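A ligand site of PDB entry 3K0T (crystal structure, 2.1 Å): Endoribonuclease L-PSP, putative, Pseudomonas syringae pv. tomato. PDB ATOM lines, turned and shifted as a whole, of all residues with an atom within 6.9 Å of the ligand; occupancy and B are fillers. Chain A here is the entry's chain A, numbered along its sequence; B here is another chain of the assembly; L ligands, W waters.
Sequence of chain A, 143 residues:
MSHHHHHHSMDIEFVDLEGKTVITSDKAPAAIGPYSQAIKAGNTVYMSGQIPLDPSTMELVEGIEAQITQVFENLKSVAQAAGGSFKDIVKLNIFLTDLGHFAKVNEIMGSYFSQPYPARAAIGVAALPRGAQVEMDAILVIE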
ATOM      1  N   ALA A  30     -32.183 -16.296  13.062  1.00  0.00           N
ATOM      2  CA  ALA A  30     -30.786 -16.707  13.231  1.00  0.00           C
ATOM      3  C   ALA A  30     -29.905 -15.452  13.325  1.00  0.00           C
ATOM      4  O   ALA A  30     -30.149 -14.472  12.609  1.00  0.00           O
ATOM      5  CB  ALA A  30     -30.342 -17.569  12.043  1.00  0.00           C
ATOM      6  N   ALA A  31     -28.912 -15.494  14.218  1.00  0.00           N
ATOM      7  CA  ALA A  31     -27.955 -14.410  14.382  1.00  0.00           C
ATOM      8  C   ALA A  31     -26.699 -14.811  13.599  1.00  0.00           C
ATOM      9  O   ALA A  31     -25.824 -15.512  14.109  1.00  0.00           O
ATOM     10  CB  ALA A  31     -27.603 -14.231  15.871  1.00  0.00           C
ATOM     11  N   ILE A  32     -26.639 -14.381  12.351  1.00  0.00           N
ATOM     12  CA  ILE A  32     -25.503 -14.681  11.497  1.00  0.00           C
ATOM     13  C   ILE A  32     -24.632 -13.440  11.524  1.00  0.00           C
ATOM     14  O   ILE A  32     -25.062 -12.353  11.150  1.00  0.00           O
ATOM     15  CB  ILE A  32     -26.008 -15.023  10.061  1.00  0.00           C
ATOM     16  CG1 ILE A  32     -26.923 -16.249  10.129  1.00  0.00           C
ATOM     17  CG2 ILE A  32     -24.835 -15.246   9.104  1.00  0.00           C
ATOM     18  CD1 ILE A  32     -26.324 -17.453  10.882  1.00  0.00           C
ATOM     19  N   GLY A  33     -23.413 -13.607  12.009  1.00  0.00           N
ATOM     20  CA  GLY A  33     -22.551 -12.451  12.123  1.00  0.00           C
ATOM     21  C   GLY A  33     -21.980 -12.407  13.522  1.00  0.00           C
ATOM     22  O   GLY A  33     -22.296 -13.251  14.350  1.00  0.00           O
ATOM     23  N   TYR A  35     -22.570 -11.363  16.546  1.00  0.00           N
ATOM     24  CA  TYR A  35     -23.426 -10.913  17.639  1.00  0.00           C
ATOM     25  C   TYR A  35     -24.292 -12.070  18.111  1.00  0.00           C
ATOM     26  O   TYR A  35     -24.445 -13.069  17.409  1.00  0.00           O
ATOM     27  CB  TYR A  35     -24.348  -9.761  17.208  1.00  0.00           C
ATOM     28  CG  TYR A  35     -25.412 -10.150  16.202  1.00  0.00           C
ATOM     29  CD1 TYR A  35     -26.768 -10.224  16.571  1.00  0.00           C
ATOM     30  CD2 TYR A  35     -25.074 -10.452  14.881  1.00  0.00           C
ATOM     31  CE1 TYR A  35     -27.760 -10.570  15.627  1.00  0.00           C
ATOM     32  CE2 TYR A  35     -26.052 -10.797  13.936  1.00  0.00           C
ATOM     33  CZ  TYR A  35     -27.387 -10.852  14.320  1.00  0.00           C
ATOM     34  OH  TYR A  35     -28.352 -11.183  13.379  1.00  0.00           O
ATOM     35  N   SER A  36     -24.874 -11.925  19.303  1.00  0.00           N
ATOM     36  CA  SER A  36     -25.768 -12.964  19.841  1.00  0.00           C
ATOM     37  C   SER A  36     -27.168 -12.381  19.967  1.00  0.00           C
ATOM     38  O   SER A  36     -27.321 -11.164  20.072  1.00  0.00           O
ATOM     39  CB  SER A  36     -25.292 -13.410  21.225  1.00  0.00           C
ATOM     40  OG  SER A  36     -23.948 -13.855  21.184  1.00  0.00           O
ATOM     41  N   SER A  48     -30.497  -8.054  21.783  1.00  0.00           N
ATOM     42  CA  SER A  48     -30.186  -7.398  20.537  1.00  0.00           C
ATOM     43  C   SER A  48     -31.416  -6.776  19.937  1.00  0.00           C
ATOM     44  O   SER A  48     -32.543  -7.158  20.261  1.00  0.00           O
ATOM     45  CB  SER A  48     -29.611  -8.401  19.531  1.00  0.00           C
ATOM     46  OG  SER A  48     -28.285  -8.765  19.873  1.00  0.00           O
ATOM     47  N   GLY A  49     -31.192  -5.829  19.037  1.00  0.00           N
ATOM     48  CA  GLY A  49     -32.286  -5.198  18.352  1.00  0.00           C
ATOM     49  C   GLY A  49     -32.895  -6.292  17.501  1.00  0.00           C
ATOM     50  O   GLY A  49     -32.184  -7.139  16.942  1.00  0.00           O
ATOM     51  N   GLN A  50     -34.215  -6.297  17.433  1.00  0.00           N
ATOM     52  CA  GLN A  50     -34.896  -7.276  16.608  1.00  0.00           C
ATOM     53  C   GLN A  50     -35.615  -6.518  15.507  1.00  0.00           C
ATOM     54  O   GLN A  50     -36.228  -5.484  15.750  1.00  0.00           O
ATOM     55  CB  GLN A  50     -35.897  -8.078  17.453  1.00  0.00           C
ATOM     56  CG  GLN A  50     -35.270  -9.184  18.312  1.00  0.00           C
ATOM     57  CD  GLN A  50     -34.660 -10.309  17.483  1.00  0.00           C
ATOM     58  OE1 GLN A  50     -35.100 -10.587  16.361  1.00  0.00           O
ATOM     59  NE2 GLN A  50     -33.656 -10.986  18.032  1.00  0.00           N
ATOM     60  N   ILE A  51     -35.503  -7.023  14.274  1.00  0.00           N
ATOM     61  CA  ILE A  51     -36.211  -6.411  13.163  1.00  0.00           C
ATOM     62  C   ILE A  51     -37.322  -7.370  12.748  1.00  0.00           C
ATOM     63  O   ILE A  51     -37.387  -8.502  13.227  1.00  0.00           O
ATOM     64  CB  ILE A  51     -35.275  -6.057  11.942  1.00  0.00           C
ATOM     65  CG1 ILE A  51     -34.379  -7.247  11.574  1.00  0.00           C
ATOM     66  CG2 ILE A  51     -34.464  -4.813  12.263  1.00  0.00           C
ATOM     67  CD1 ILE A  51     -33.593  -7.036  10.264  1.00  0.00           C
ATOM     68  N   LEU A  53     -38.057  -9.743  10.913  1.00  0.00           N
ATOM     69  CA  LEU A  53     -37.717 -10.921  10.123  1.00  0.00           C
ATOM     70  C   LEU A  53     -38.579 -12.103  10.521  1.00  0.00           C
ATOM     71  O   LEU A  53     -38.779 -12.358  11.696  1.00  0.00           O
ATOM     72  CB  LEU A  53     -36.240 -11.299  10.360  1.00  0.00           C
ATOM     73  CG  LEU A  53     -35.128 -10.548   9.636  1.00  0.00           C
ATOM     74  CD1 LEU A  53     -33.769 -10.918  10.249  1.00  0.00           C
ATOM     75  CD2 LEU A  53     -35.158 -10.900   8.162  1.00  0.00           C
ATOM     76  N   MET A  58     -36.506 -15.687   6.756  1.00  0.00           N
ATOM     77  CA  MET A  58     -35.466 -14.662   6.806  1.00  0.00           C
ATOM     78  C   MET A  58     -35.715 -13.493   5.817  1.00  0.00           C
ATOM     79  O   MET A  58     -34.777 -12.915   5.250  1.00  0.00           O
ATOM     80  CB  MET A  58     -34.059 -15.261   6.663  1.00  0.00           C
ATOM     81  CG  MET A  58     -33.684 -16.150   7.878  1.00  0.00           C
ATOM     82  SD  MET A  58     -33.712 -15.239   9.631  1.00  0.00           S
ATOM     83  CE  MET A  58     -32.008 -14.354   9.430  1.00  0.00           C
ATOM     84  N   PRO A 129     -31.886  -1.640   9.243  1.00  0.00           N
ATOM     85  CA  PRO A 129     -31.352  -2.798   8.495  1.00  0.00           C
ATOM     86  C   PRO A 129     -32.414  -3.496   7.656  1.00  0.00           C
ATOM     87  O   PRO A 129     -33.546  -3.718   8.122  1.00  0.00           O
ATOM     88  CB  PRO A 129     -30.832  -3.721   9.599  1.00  0.00           C
ATOM     89  CG  PRO A 129     -30.383  -2.749  10.678  1.00  0.00           C
ATOM     90  CD  PRO A 129     -31.490  -1.692  10.667  1.00  0.00           C
ATOM     91  N   ARG A 130     -32.061  -3.834   6.417  1.00  0.00           N
ATOM     92  CA  ARG A 130     -32.950  -4.549   5.471  1.00  0.00           C
ATOM     93  C   ARG A 130     -34.184  -3.788   4.984  1.00  0.00           C
ATOM     94  O   ARG A 130     -35.064  -4.367   4.373  1.00  0.00           O
ATOM     95  CB  ARG A 130     -33.388  -5.894   6.059  1.00  0.00           C
ATOM     96  CG  ARG A 130     -32.225  -6.679   6.618  1.00  0.00           C
ATOM     97  CD  ARG A 130     -32.511  -8.162   6.738  1.00  0.00           C
ATOM     98  NE  ARG A 130     -31.586  -8.778   7.689  1.00  0.00           N
ATOM     99  CZ  ARG A 130     -31.189 -10.043   7.651  1.00  0.00           C
ATOM    100  NH1 ARG A 130     -31.632 -10.844   6.685  1.00  0.00           N
ATOM    101  NH2 ARG A 130     -30.356 -10.512   8.577  1.00  0.00           N
ATOM    102  N   GLU A 135     -37.566  -1.412  14.496  1.00  0.00           N
ATOM    103  CA  GLU A 135     -36.570  -2.241  15.173  1.00  0.00           C
ATOM    104  C   GLU A 135     -36.737  -1.903  16.651  1.00  0.00           C
ATOM    105  O   GLU A 135     -37.039  -0.756  17.011  1.00  0.00           O
ATOM    106  CB  GLU A 135     -35.140  -1.890  14.757  1.00  0.00           C
ATOM    107  CG  GLU A 135     -34.046  -2.702  15.548  1.00  0.00           C
ATOM    108  CD  GLU A 135     -32.628  -2.412  15.090  1.00  0.00           C
ATOM    109  OE1 GLU A 135     -32.470  -1.727  14.050  1.00  0.00           O
ATOM    110  OE2 GLU A 135     -31.658  -2.866  15.742  1.00  0.00           O
ATOM    111  N   MET A 136     -36.568  -2.907  17.504  1.00  0.00           N
ATOM    112  CA  MET A 136     -36.665  -2.689  18.933  1.00  0.00           C
ATOM    113  C   MET A 136     -35.673  -3.573  19.676  1.00  0.00           C
ATOM    114  O   MET A 136     -35.432  -4.707  19.273  1.00  0.00           O
ATOM    115  CB  MET A 136     -38.074  -3.019  19.461  1.00  0.00           C
ATOM    116  CG  MET A 136     -39.185  -2.090  19.011  1.00  0.00           C
ATOM    117  SD  MET A 136     -40.913  -2.602  19.761  1.00  0.00           S
ATOM    118  CE  MET A 136     -41.779  -3.198  18.131  1.00  0.00           C
ATOM    119  N   ILE B  94     -24.695   0.282  17.142  1.00  0.00           N
ATOM    120  CA  ILE B  94     -24.080   0.816  15.931  1.00  0.00           C
ATOM    121  C   ILE B  94     -24.975   1.892  15.278  1.00  0.00           C
ATOM    122  O   ILE B  94     -26.140   1.634  14.957  1.00  0.00           O
ATOM    123  CB  ILE B  94     -23.803  -0.305  14.890  1.00  0.00           C
ATOM    124  CG1 ILE B  94     -22.720  -1.270  15.414  1.00  0.00           C
ATOM    125  CG2 ILE B  94     -23.358   0.306  13.562  1.00  0.00           C
ATOM    126  CD1 ILE B  94     -22.848  -2.690  14.860  1.00  0.00           C
ATOM    127  N   PHE B 102     -23.102  -1.348   6.360  1.00  0.00           N
ATOM    128  CA  PHE B 102     -23.262  -2.321   7.447  1.00  0.00           C
ATOM    129  C   PHE B 102     -22.426  -3.597   7.246  1.00  0.00           C
ATOM    130  O   PHE B 102     -21.825  -4.084   8.199  1.00  0.00           O
ATOM    131  CB  PHE B 102     -24.751  -2.629   7.650  1.00  0.00           C
ATOM    132  CG  PHE B 102     -25.061  -3.342   8.950  1.00  0.00           C
ATOM    133  CD1 PHE B 102     -24.424  -2.984  10.135  1.00  0.00           C
ATOM    134  CD2 PHE B 102     -25.997  -4.358   8.978  1.00  0.00           C
ATOM    135  CE1 PHE B 102     -24.718  -3.641  11.325  1.00  0.00           C
ATOM    136  CE2 PHE B 102     -26.296  -5.026  10.176  1.00  0.00           C
ATOM    137  CZ  PHE B 102     -25.653  -4.670  11.348  1.00  0.00           C
ATOM    138  N   ASN B 106     -19.786  -5.343   9.913  1.00  0.00           N
ATOM    139  CA  ASN B 106     -19.792  -6.770  10.261  1.00  0.00           C
ATOM    140  C   ASN B 106     -18.447  -7.434  10.058  1.00  0.00           C
ATOM    141  O   ASN B 106     -17.965  -8.165  10.935  1.00  0.00           O
ATOM    142  CB  ASN B 106     -20.815  -7.514   9.413  1.00  0.00           C
ATOM    143  CG  ASN B 106     -22.209  -7.421   9.962  1.00  0.00           C
ATOM    144  OD1 ASN B 106     -23.161  -7.157   9.230  1.00  0.00           O
ATOM    145  ND2 ASN B 106     -22.335  -7.624  11.255  1.00  0.00           N
ATOM    146  N   ALA B 119     -24.487  -8.705  22.366  1.00  0.00           N
ATOM    147  CA  ALA B 119     -25.796  -8.391  21.792  1.00  0.00           C
ATOM    148  C   ALA B 119     -25.527  -7.090  21.066  1.00  0.00           C
ATOM    149  O   ALA B 119     -24.568  -6.388  21.415  1.00  0.00           O
ATOM    150  CB  ALA B 119     -26.825  -8.160  22.898  1.00  0.00           C
ATOM    151  N   ARG B 120     -26.318  -6.750  20.069  1.00  0.00           N
ATOM    152  CA  ARG B 120     -26.114  -5.464  19.418  1.00  0.00           C
ATOM    153  C   ARG B 120     -27.382  -4.952  18.740  1.00  0.00           C
ATOM    154  O   ARG B 120     -28.334  -5.711  18.530  1.00  0.00           O
ATOM    155  CB  ARG B 120     -24.945  -5.507  18.419  1.00  0.00           C
ATOM    156  CG  ARG B 120     -25.339  -6.011  17.053  1.00  0.00           C
ATOM    157  CD  ARG B 120     -24.182  -6.145  16.075  1.00  0.00           C
ATOM    158  NE  ARG B 120     -24.730  -6.793  14.897  1.00  0.00           N
ATOM    159  CZ  ARG B 120     -24.032  -7.190  13.838  1.00  0.00           C
ATOM    160  NH1 ARG B 120     -22.721  -7.008  13.789  1.00  0.00           N
ATOM    161  NH2 ARG B 120     -24.671  -7.790  12.845  1.00  0.00           N
ATOM    162  N   ALA B 121     -27.391  -3.650  18.446  1.00  0.00           N
ATOM    163  CA  ALA B 121     -28.493  -3.010  17.754  1.00  0.00           C
ATOM    164  C   ALA B 121     -27.807  -2.190  16.680  1.00  0.00           C
ATOM    165  O   ALA B 121     -26.640  -1.834  16.834  1.00  0.00           O
ATOM    166  CB  ALA B 121     -29.304  -2.108  18.705  1.00  0.00           C
ATOM    167  N   ALA B 122     -28.522  -1.896  15.595  1.00  0.00           N
ATOM    168  CA  ALA B 122     -27.917  -1.137  14.507  1.00  0.00           C
ATOM    169  C   ALA B 122     -28.998  -0.324  13.822  1.00  0.00           C
ATOM    170  O   ALA B 122     -29.997  -0.878  13.369  1.00  0.00           O
ATOM    171  CB  ALA B 122     -27.253  -2.098  13.507  1.00  0.00           C
HETATM  172  C1  LIG L   1     -29.773  -7.138  14.530  1.00  0.00           C
HETATM  173  C2  LIG L   1     -28.379  -7.064  13.977  1.00  0.00           C
HETATM  174  C3  LIG L   1     -28.498  -7.886  12.706  1.00  0.00           C
HETATM  175  C4  LIG L   1     -29.617  -7.307  11.782  1.00  0.00           C
HETATM  176  C5  LIG L   1     -30.107  -8.229  10.704  1.00  0.00           C
HETATM  177  C6  LIG L   1     -30.483  -6.136  13.674  1.00  0.00           C
HETATM  178  O1  LIG L   1     -31.654  -5.710  14.277  1.00  0.00           O
HETATM  179  O2  LIG L   1     -29.882  -6.824  15.898  1.00  0.00           O
HETATM  180  O3  LIG L   1     -27.430  -7.571  14.900  1.00  0.00           O
HETATM  181  O4  LIG L   1     -27.268  -7.832  12.012  1.00  0.00           O
HETATM  182  O5  LIG L   1     -30.801  -6.826  12.481  1.00  0.00           O
HETATM  183  O6  LIG L   1     -30.027  -7.476   9.525  1.00  0.00           O
HETATM  184  O   HOH W   1     -28.195  -7.450   7.549  1.00  0.00           O
HETATM  185  O   HOH W   2     -31.775  -9.643  13.387  1.00  0.00           O
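O of Gly 49 lies within hydrogen-bond range of O2 of the ligand, at 2.5 Å.
The backbone carbonyl oxygen (O) of Arg 120 of chain B lies within hydrogen-bond range of an oxygen (O2) of the ligand, 3.2 Å away.
The guanidinium group (NH2) of Arg 120 of chain B lies within hydrogen-bond range of an oxygen (O4) of the ligand (2.7 Å).
NE of Arg 130 sits at hydrogen-bond distance from O6 of the ligand (2.7 Å).
The side-chain carboxylate (OE2) of Glu 135 is in hydrogen-bond range of an oxygen (O1) of the ligand (3.2 Å).
Residues that only touch the ligand: Tyr 35 (3.1 Å), Ser 48 (3.97 Å), Ile 51 (3.6 Å), Pro 129 (3.8 Å) and Phe 102 of chain B (3.5 Å).
Hydrophobic or aromatic side chains that line the ligand: Tyr 35, Ile 51, Pro 129 and Phe 102 of chain B.
Within 4 Å of the ligand: Tyr 35, Ser 48, Gly 49, Ile 51, Pro 129, Arg 130, Glu 135, Phe 102 of chain B and Arg 120 of chain B.
O of Arg 120 of chain B is in hydrogen-bond range of N of Gly 49, 2.9 Å away.
N of Arg 120 of chain B is in hydrogen-bond range of OG of Ser 48 (2.8 Å).
The side-chain amide nitrogen (ND2) of Asn 106 of chain B lies close to the guanidinium group (NH1) of Arg 120 of chain B, at 2.6 Å.
The backbone NH of Ala 122 of chain B is in hydrogen-bond range of the side-chain carboxylate of Glu 135 (3.3 Å).
The side-chain hydroxyl (OG) of Ser 48 sits at hydrogen-bond distance from the backbone carbonyl oxygen (O) of Ser 36 (2.6 Å).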
